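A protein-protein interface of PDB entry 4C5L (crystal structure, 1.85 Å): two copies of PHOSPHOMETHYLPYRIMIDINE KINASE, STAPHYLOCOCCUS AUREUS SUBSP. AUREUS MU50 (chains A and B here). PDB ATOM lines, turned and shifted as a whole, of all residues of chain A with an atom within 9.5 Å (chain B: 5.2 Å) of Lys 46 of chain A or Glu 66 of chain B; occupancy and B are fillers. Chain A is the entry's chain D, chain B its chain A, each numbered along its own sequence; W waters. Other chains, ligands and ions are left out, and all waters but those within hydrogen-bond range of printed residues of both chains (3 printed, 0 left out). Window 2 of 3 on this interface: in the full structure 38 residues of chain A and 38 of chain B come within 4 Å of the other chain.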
ATOM      1  N   THR A  14      13.897  18.657 -25.110  1.00  0.00           N
ATOM      2  CA  THR A  14      13.548  19.053 -26.466  1.00  0.00           C
ATOM      3  C   THR A  14      13.476  20.573 -26.630  1.00  0.00           C
ATOM      4  O   THR A  14      13.833  21.091 -27.665  1.00  0.00           O
ATOM      5  CB  THR A  14      12.290  18.335 -26.977  1.00  0.00           C
ATOM      6  OG1 THR A  14      12.496  16.932 -26.885  1.00  0.00           O
ATOM      7  CG2 THR A  14      12.014  18.703 -28.413  1.00  0.00           C
ATOM      8  N   SER A  15      13.053  21.274 -25.588  1.00  0.00           N
ATOM      9  CA  SER A  15      12.936  22.741 -25.652  1.00  0.00           C
ATOM     10  C   SER A  15      14.312  23.441 -25.773  1.00  0.00           C
ATOM     11  O   SER A  15      14.401  24.589 -26.215  1.00  0.00           O
ATOM     12  CB  SER A  15      12.036  23.277 -24.507  1.00  0.00           C
ATOM     13  OG  SER A  15      12.701  23.211 -23.253  1.00  0.00           O
ATOM     14  N   THR A  43       9.978  15.590 -23.761  1.00  0.00           N
ATOM     15  CA  THR A  43       9.147  16.361 -24.690  1.00  0.00           C
ATOM     16  C   THR A  43       8.082  17.103 -23.903  1.00  0.00           C
ATOM     17  O   THR A  43       7.853  16.807 -22.731  1.00  0.00           O
ATOM     18  CB  THR A  43       8.502  15.483 -25.793  1.00  0.00           C
ATOM     19  OG1 THR A  43       7.756  14.398 -25.210  1.00  0.00           O
ATOM     20  CG2 THR A  43       9.611  14.886 -26.679  1.00  0.00           C
ATOM     21  N   MET A  44       7.444  18.067 -24.563  1.00  0.00           N
ATOM     22  CA  MET A  44       6.425  18.900 -23.946  1.00  0.00           C
ATOM     23  C   MET A  44       5.248  19.040 -24.886  1.00  0.00           C
ATOM     24  O   MET A  44       5.440  19.231 -26.076  1.00  0.00           O
ATOM     25  CB  MET A  44       6.993  20.303 -23.658  1.00  0.00           C
ATOM     26  CG  MET A  44       8.152  20.362 -22.684  1.00  0.00           C
ATOM     27  SD  MET A  44       9.748  19.892 -23.378  1.00  0.00           S
ATOM     28  CE  MET A  44      10.784  20.110 -21.935  1.00  0.00           C
ATOM     29  N   ASP A  45       4.037  19.001 -24.340  1.00  0.00           N
ATOM     30  CA  ASP A  45       2.829  19.072 -25.149  1.00  0.00           C
ATOM     31  C   ASP A  45       2.634  20.511 -25.633  1.00  0.00           C
ATOM     32  O   ASP A  45       2.931  21.452 -24.903  1.00  0.00           O
ATOM     33  CB  ASP A  45       1.616  18.583 -24.346  1.00  0.00           C
ATOM     34  CG  ASP A  45       0.338  18.843 -25.051  1.00  0.00           C
ATOM     35  OD1 ASP A  45      -0.148  19.988 -24.988  1.00  0.00           O
ATOM     36  OD2 ASP A  45      -0.175  17.916 -25.702  1.00  0.00           O
ATOM     37  N   LYS A  46       2.131  20.683 -26.856  1.00  0.00           N
ATOM     38  CA  LYS A  46       2.189  21.997 -27.506  1.00  0.00           C
ATOM     39  C   LYS A  46       1.262  23.020 -26.854  1.00  0.00           C
ATOM     40  O   LYS A  46       1.525  24.221 -26.901  1.00  0.00           O
ATOM     41  CB  LYS A  46       1.903  21.896 -29.009  1.00  0.00           C
ATOM     42  CG  LYS A  46       0.563  21.274 -29.402  1.00  0.00           C
ATOM     43  CD  LYS A  46       0.339  21.332 -30.908  1.00  0.00           C
ATOM     44  CE  LYS A  46      -0.801  20.415 -31.344  1.00  0.00           C
ATOM     45  NZ  LYS A  46      -1.712  21.077 -32.319  1.00  0.00           N
ATOM     46  N   ASP A  47       0.205  22.526 -26.240  1.00  0.00           N
ATOM     47  CA  ASP A  47      -0.858  23.365 -25.693  1.00  0.00           C
ATOM     48  C   ASP A  47      -0.761  23.597 -24.195  1.00  0.00           C
ATOM     49  O   ASP A  47      -1.254  24.615 -23.707  1.00  0.00           O
ATOM     50  CB  ASP A  47      -2.224  22.699 -25.926  1.00  0.00           C
ATOM     51  CG  ASP A  47      -2.584  22.623 -27.366  1.00  0.00           C
ATOM     52  OD1 ASP A  47      -2.283  23.594 -28.078  1.00  0.00           O
ATOM     53  OD2 ASP A  47      -3.208  21.618 -27.780  1.00  0.00           O
ATOM     54  N   THR A  48      -0.228  22.612 -23.476  1.00  0.00           N
ATOM     55  CA  THR A  48      -0.264  22.580 -22.001  1.00  0.00           C
ATOM     56  C   THR A  48       1.127  22.623 -21.382  1.00  0.00           C
ATOM     57  O   THR A  48       1.275  22.921 -20.197  1.00  0.00           O
ATOM     58  CB  THR A  48      -0.885  21.256 -21.496  1.00  0.00           C
ATOM     59  OG1 THR A  48       0.039  20.183 -21.733  1.00  0.00           O
ATOM     60  CG2 THR A  48      -2.211  20.941 -22.175  1.00  0.00           C
ATOM     61  N   TRP A  49       2.127  22.280 -22.204  1.00  0.00           N
ATOM     62  CA  TRP A  49       3.535  22.105 -21.808  1.00  0.00           C
ATOM     63  C   TRP A  49       3.829  20.930 -20.844  1.00  0.00           C
ATOM     64  O   TRP A  49       4.942  20.834 -20.341  1.00  0.00           O
ATOM     65  CB  TRP A  49       4.158  23.437 -21.299  1.00  0.00           C
ATOM     66  CG  TRP A  49       5.566  23.637 -21.806  1.00  0.00           C
ATOM     67  CD1 TRP A  49       6.704  23.763 -21.069  1.00  0.00           C
ATOM     68  CD2 TRP A  49       5.965  23.711 -23.179  1.00  0.00           C
ATOM     69  NE1 TRP A  49       7.779  23.952 -21.895  1.00  0.00           N
ATOM     70  CE2 TRP A  49       7.362  23.891 -23.200  1.00  0.00           C
ATOM     71  CE3 TRP A  49       5.272  23.637 -24.397  1.00  0.00           C
ATOM     72  CZ2 TRP A  49       8.080  23.998 -24.384  1.00  0.00           C
ATOM     73  CZ3 TRP A  49       5.982  23.744 -25.572  1.00  0.00           C
ATOM     74  CH2 TRP A  49       7.377  23.927 -25.558  1.00  0.00           C
ATOM     75  N   SER A  50       2.873  20.016 -20.623  1.00  0.00           N
ATOM     76  CA  SER A  50       3.126  18.874 -19.720  1.00  0.00           C
ATOM     77  C   SER A  50       4.307  18.119 -20.264  1.00  0.00           C
ATOM     78  O   SER A  50       4.416  17.959 -21.475  1.00  0.00           O
ATOM     79  CB  SER A  50       1.941  17.890 -19.596  1.00  0.00           C
ATOM     80  OG  SER A  50       0.709  18.553 -19.724  1.00  0.00           O
ATOM     81  N   HIS A  51       5.189  17.688 -19.358  1.00  0.00           N
ATOM     82  CA  HIS A  51       6.396  16.978 -19.708  1.00  0.00           C
ATOM     83  C   HIS A  51       6.123  15.472 -19.864  1.00  0.00           C
ATOM     84  O   HIS A  51       5.268  14.912 -19.174  1.00  0.00           O
ATOM     85  CB  HIS A  51       7.440  17.184 -18.632  1.00  0.00           C
ATOM     86  CG  HIS A  51       8.091  18.527 -18.674  1.00  0.00           C
ATOM     87  ND1 HIS A  51       7.391  19.696 -18.921  1.00  0.00           N
ATOM     88  CD2 HIS A  51       9.373  18.892 -18.452  1.00  0.00           C
ATOM     89  CE1 HIS A  51       8.228  20.719 -18.868  1.00  0.00           C
ATOM     90  NE2 HIS A  51       9.440  20.251 -18.603  1.00  0.00           N
ATOM     91  N   ASP A  52       6.846  14.842 -20.786  1.00  0.00           N
ATOM     92  CA  ASP A  52       6.815  13.397 -20.984  1.00  0.00           C
ATOM     93  C   ASP A  52       8.268  12.983 -21.004  1.00  0.00           C
ATOM     94  O   ASP A  52       9.051  13.551 -21.777  1.00  0.00           O
ATOM     95  CB  ASP A  52       6.175  13.085 -22.329  1.00  0.00           C
ATOM     96  CG  ASP A  52       5.863  11.621 -22.520  1.00  0.00           C
ATOM     97  OD1 ASP A  52       6.425  10.756 -21.814  1.00  0.00           O
ATOM     98  OD2 ASP A  52       4.971  11.311 -23.335  1.00  0.00           O
ATOM     99  N   MET A 251       9.750  32.037 -24.275  1.00  0.00           N
ATOM    100  CA  MET A 251       9.581  30.997 -25.299  1.00  0.00           C
ATOM    101  C   MET A 251       8.112  30.747 -25.575  1.00  0.00           C
ATOM    102  O   MET A 251       7.720  30.534 -26.734  1.00  0.00           O
ATOM    103  CB  MET A 251      10.234  29.698 -24.852  1.00  0.00           C
ATOM    104  CG  MET A 251       9.877  28.493 -25.713  1.00  0.00           C
ATOM    105  SD  MET A 251      10.922  27.096 -25.329  1.00  0.00           S
ATOM    106  CE  MET A 251      12.471  27.580 -26.087  1.00  0.00           C
ATOM    107  N   ASN A 252       7.327  30.703 -24.508  1.00  0.00           N
ATOM    108  CA  ASN A 252       5.870  30.650 -24.625  1.00  0.00           C
ATOM    109  C   ASN A 252       5.270  31.108 -23.294  1.00  0.00           C
ATOM    110  O   ASN A 252       5.944  31.707 -22.465  1.00  0.00           O
ATOM    111  CB  ASN A 252       5.416  29.222 -25.010  1.00  0.00           C
ATOM    112  CG  ASN A 252       5.999  28.173 -24.096  1.00  0.00           C
ATOM    113  OD1 ASN A 252       6.035  28.352 -22.883  1.00  0.00           O
ATOM    114  ND2 ASN A 252       6.496  27.084 -24.663  1.00  0.00           N
ATOM    115  N   ASP A 253       3.999  30.803 -23.100  1.00  0.00           N
ATOM    116  CA  ASP A 253       3.257  31.227 -21.912  1.00  0.00           C
ATOM    117  C   ASP A 253       3.722  30.570 -20.616  1.00  0.00           C
ATOM    118  O   ASP A 253       3.381  31.041 -19.528  1.00  0.00           O
ATOM    119  CB  ASP A 253       1.781  30.917 -22.131  1.00  0.00           C
ATOM    120  CG  ASP A 253       1.103  31.930 -23.015  1.00  0.00           C
ATOM    121  OD1 ASP A 253       1.618  33.069 -23.123  1.00  0.00           O
ATOM    122  OD2 ASP A 253       0.024  31.607 -23.553  1.00  0.00           O
ATOM    123  N   PHE A 254       4.511  29.501 -20.736  1.00  0.00           N
ATOM    124  CA  PHE A 254       4.883  28.659 -19.608  1.00  0.00           C
ATOM    125  C   PHE A 254       6.332  28.808 -19.191  1.00  0.00           C
ATOM    126  O   PHE A 254       6.658  28.579 -18.026  1.00  0.00           O
ATOM    127  CB  PHE A 254       4.666  27.191 -19.968  1.00  0.00           C
ATOM    128  CG  PHE A 254       3.265  26.874 -20.407  1.00  0.00           C
ATOM    129  CD1 PHE A 254       2.284  26.622 -19.477  1.00  0.00           C
ATOM    130  CD2 PHE A 254       2.944  26.825 -21.759  1.00  0.00           C
ATOM    131  CE1 PHE A 254       0.990  26.325 -19.872  1.00  0.00           C
ATOM    132  CE2 PHE A 254       1.669  26.522 -22.175  1.00  0.00           C
ATOM    133  CZ  PHE A 254       0.683  26.284 -21.233  1.00  0.00           C
ATOM    134  N   GLU B  62       8.033  11.936 -33.138  1.00  0.00           N
ATOM    135  CA  GLU B  62       6.910  12.839 -33.364  1.00  0.00           C
ATOM    136  C   GLU B  62       6.577  13.764 -32.187  1.00  0.00           C
ATOM    137  O   GLU B  62       6.000  14.845 -32.388  1.00  0.00           O
ATOM    138  CB  GLU B  62       5.652  12.021 -33.690  1.00  0.00           C
ATOM    139  CG  GLU B  62       5.694  11.259 -35.009  1.00  0.00           C
ATOM    140  CD  GLU B  62       5.435  12.139 -36.220  1.00  0.00           C
ATOM    141  OE1 GLU B  62       5.119  13.338 -36.055  1.00  0.00           O
ATOM    142  OE2 GLU B  62       5.518  11.620 -37.359  1.00  0.00           O
ATOM    143  N   LYS B  63       6.831  13.308 -30.971  1.00  0.00           N
ATOM    144  CA  LYS B  63       6.631  14.144 -29.783  1.00  0.00           C
ATOM    145  C   LYS B  63       7.674  15.283 -29.752  1.00  0.00           C
ATOM    146  O   LYS B  63       7.377  16.415 -29.382  1.00  0.00           O
ATOM    147  CB  LYS B  63       6.744  13.293 -28.532  1.00  0.00           C
ATOM    148  CG  LYS B  63       5.535  12.383 -28.282  1.00  0.00           C
ATOM    149  CD  LYS B  63       5.672  11.678 -26.942  1.00  0.00           C
ATOM    150  CE  LYS B  63       5.088  10.281 -27.003  1.00  0.00           C
ATOM    151  NZ  LYS B  63       5.089   9.604 -25.677  1.00  0.00           N
ATOM    152  N   GLN B  64       8.903  14.955 -30.119  1.00  0.00           N
ATOM    153  CA  GLN B  64       9.950  15.947 -30.278  1.00  0.00           C
ATOM    154  C   GLN B  64       9.640  16.997 -31.346  1.00  0.00           C
ATOM    155  O   GLN B  64       9.916  18.178 -31.146  1.00  0.00           O
ATOM    156  CB  GLN B  64      11.253  15.259 -30.654  1.00  0.00           C
ATOM    157  CG  GLN B  64      11.872  14.433 -29.552  1.00  0.00           C
ATOM    158  CD  GLN B  64      13.160  13.855 -30.055  1.00  0.00           C
ATOM    159  OE1 GLN B  64      14.193  14.497 -29.981  1.00  0.00           O
ATOM    160  NE2 GLN B  64      13.079  12.689 -30.706  1.00  0.00           N
ATOM    161  N   LEU B  65       9.122  16.555 -32.494  1.00  0.00           N
ATOM    162  CA  LEU B  65       8.693  17.468 -33.549  1.00  0.00           C
ATOM    163  C   LEU B  65       7.559  18.391 -33.091  1.00  0.00           C
ATOM    164  O   LEU B  65       7.611  19.604 -33.339  1.00  0.00           O
ATOM    165  CB  LEU B  65       8.247  16.704 -34.794  1.00  0.00           C
ATOM    166  CG  LEU B  65       9.322  15.916 -35.553  1.00  0.00           C
ATOM    167  CD1 LEU B  65       8.726  15.430 -36.864  1.00  0.00           C
ATOM    168  CD2 LEU B  65      10.576  16.735 -35.806  1.00  0.00           C
ATOM    169  N   GLU B  66       6.555  17.833 -32.416  1.00  0.00           N
ATOM    170  CA  GLU B  66       5.493  18.651 -31.852  1.00  0.00           C
ATOM    171  C   GLU B  66       5.965  19.822 -30.963  1.00  0.00           C
ATOM    172  O   GLU B  66       5.448  20.966 -31.081  1.00  0.00           O
ATOM    173  CB  GLU B  66       4.507  17.798 -31.072  1.00  0.00           C
ATOM    174  CG  GLU B  66       3.297  18.593 -30.618  1.00  0.00           C
ATOM    175  CD  GLU B  66       2.362  17.795 -29.729  1.00  0.00           C
ATOM    176  OE1 GLU B  66       1.978  16.678 -30.139  1.00  0.00           O
ATOM    177  OE2 GLU B  66       2.014  18.294 -28.627  1.00  0.00           O
ATOM    178  N   THR B  67       6.903  19.531 -30.064  1.00  0.00           N
ATOM    179  CA  THR B  67       7.492  20.531 -29.183  1.00  0.00           C
ATOM    180  C   THR B  67       8.353  21.530 -29.965  1.00  0.00           C
ATOM    181  O   THR B  67       8.293  22.714 -29.707  1.00  0.00           O
ATOM    182  CB  THR B  67       8.436  19.871 -28.153  1.00  0.00           C
ATOM    183  OG1 THR B  67       7.750  18.841 -27.433  1.00  0.00           O
ATOM    184  CG2 THR B  67       9.055  20.914 -27.192  1.00  0.00           C
ATOM    185  N   ALA B  68       9.198  21.038 -30.875  1.00  0.00           N
ATOM    186  CA  ALA B  68      10.070  21.935 -31.652  1.00  0.00           C
ATOM    187  C   ALA B  68       9.259  22.863 -32.523  1.00  0.00           C
ATOM    188  O   ALA B  68       9.601  24.039 -32.626  1.00  0.00           O
ATOM    189  CB  ALA B  68      11.118  21.168 -32.478  1.00  0.00           C
ATOM    190  N   LEU B  69       8.190  22.338 -33.109  1.00  0.00           N
ATOM    191  CA  LEU B  69       7.317  23.115 -33.960  1.00  0.00           C
ATOM    192  C   LEU B  69       6.520  24.153 -33.177  1.00  0.00           C
ATOM    193  O   LEU B  69       6.247  25.230 -33.695  1.00  0.00           O
ATOM    194  CB  LEU B  69       6.369  22.198 -34.746  1.00  0.00           C
ATOM    195  CG  LEU B  69       5.162  22.769 -35.536  1.00  0.00           C
ATOM    196  CD1 LEU B  69       5.543  23.614 -36.763  1.00  0.00           C
ATOM    197  CD2 LEU B  69       4.231  21.636 -35.993  1.00  0.00           C
ATOM    198  N   SER B  70       6.143  23.853 -31.935  1.00  0.00           N
ATOM    199  CA  SER B  70       5.380  24.838 -31.166  1.00  0.00           C
ATOM    200  C   SER B  70       6.283  26.012 -30.812  1.00  0.00           C
ATOM    201  O   SER B  70       5.834  27.109 -30.668  1.00  0.00           O
ATOM    202  CB  SER B  70       4.745  24.236 -29.893  1.00  0.00           C
ATOM    203  OG  SER B  70       5.692  24.189 -28.853  1.00  0.00           O
HETATM  204  O   HOH W   1       5.530  26.663 -27.358  1.00  0.00           O
HETATM  205  O   HOH W   2      14.822  15.903 -27.735  1.00  0.00           O
HETATM  206  O   HOH W   3       5.401  16.691 -27.708  1.00  0.00           O
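NZ of Lys 63 of chain B is in salt-bridge range of OD2 of Asp 52 of chain A, 2.9 Å away.
The side-chain carboxylate (OE2) of Glu 66 of chain B sits at hydrogen-bond distance from the backbone NH (N) of Lys 46 of chain A.
The side-chain hydroxyl (OG1) of Thr 67 of chain B lies within hydrogen-bond range of the backbone carbonyl oxygen (O) of Met 44 of chain A (2.7 Å).
The side-chain hydroxyl (OG1) of Thr 67 of chain B is in hydrogen-bond range of the backbone carbonyl oxygen (O) of Lys 63 of chain B (3.1 Å).
O of Thr 67 of chain B lies within hydrogen-bond range of OG of Ser 70 of chain B, 3.1 Å away.
The backbone carbonyl oxygen (O) of Thr 43 of chain A sits at hydrogen-bond distance from the backbone NH (N) of Asp 52 of chain A, 2.9 Å away.
The side-chain carboxylate (OD1) of Asp 45 of chain A lies within hydrogen-bond range of the backbone NH (N) of Asp 47 of chain A, 2.9 Å away.
The side-chain carboxylate (OD1) of Asp 45 of chain A sits at hydrogen-bond distance from the backbone NH (N) of Thr 48 of chain A (3.0 Å).
The backbone carbonyl oxygen of Trp 49 of chain A sits at hydrogen-bond distance from a ring nitrogen (ND1) of His 51 of chain A (3.1 Å).
Gln 64 of chain B touches Thr 14 of chain A (O to CG2, 3.5 Å).
Thr 14 of chain A touches Thr 67 of chain B.
Thr 43 of chain A touches Lys 63 of chain B (OG1 to CB, 3.6 Å).
Gln 64 of chain B touches Thr 43 of chain A (N to CG2, 3.5 Å).
Thr 43 of chain A touches Thr 67 of chain B.
CA of Asp 45 of chain A touches OE2 of Glu 66 of chain B, at 3.7 Å.
CB of Lys 46 of chain A touches CB of Ser 70 of chain B, at 3.8 Å.
Trp 49 of chain A touches Thr 67 of chain B.
Trp 49 of chain A touches Ser 70 of chain B.
Among the printed residues, 12 pairs touch across the chains.
No position is printed for both chains.
Of the printed residues of chain B, Asp 45 of chain A touches Glu 66.
Of the printed residues of chain B, Lys 46 of chain A touches Glu 66 and Ser 70.
Printed residues of chain B within 4 Å of Trp 49 of chain A: Thr 67 and Ser 70.
His 51 of chain A touches none of the printed residues of chain B.
Of the printed residues of chain B, Asp 52 of chain A touches Lys 63 (2.9 Å).
Printed residues of chain A within 4 Å of Lys 63 of chain B: Thr 43 and Asp 52.
Of the printed residues of chain A, Gln 64 of chain B touches Thr 14 (3.5 Å) and Thr 43 (3.5 Å).
Of chain A, only Asp 45 and Lys 46 come within 4 Å of Glu 66 of chain B.
Thr 67 of chain B touches just these residues of chain A: Thr 14 (3.8 Å), Thr 43 (3.8 Å), Met 44 (2.7 Å) and Trp 49 (3.8 Å).
The nearest printed residue of chain B that does not touch Lys 46 of chain A is Thr 67 of chain B (5.6 Å).
Water W3 lies within hydrogen-bond range of the backbone carbonyl oxygen (O) of Lys 63 of chain B, the backbone carbonyl oxygen (O) of Met 44 of chain A and the side-chain hydroxyl (OG1) of Thr 67 of chain B.
Water W2 lies within hydrogen-bond range of OG1 of Thr 14 of chain A (2.7 Å) and OE1 of Gln 64 of chain B (2.7 Å).
Water W1 bridges the side-chain amide nitrogen of Asn 252 of chain A and the side-chain hydroxyl of Ser 70 of chain B.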
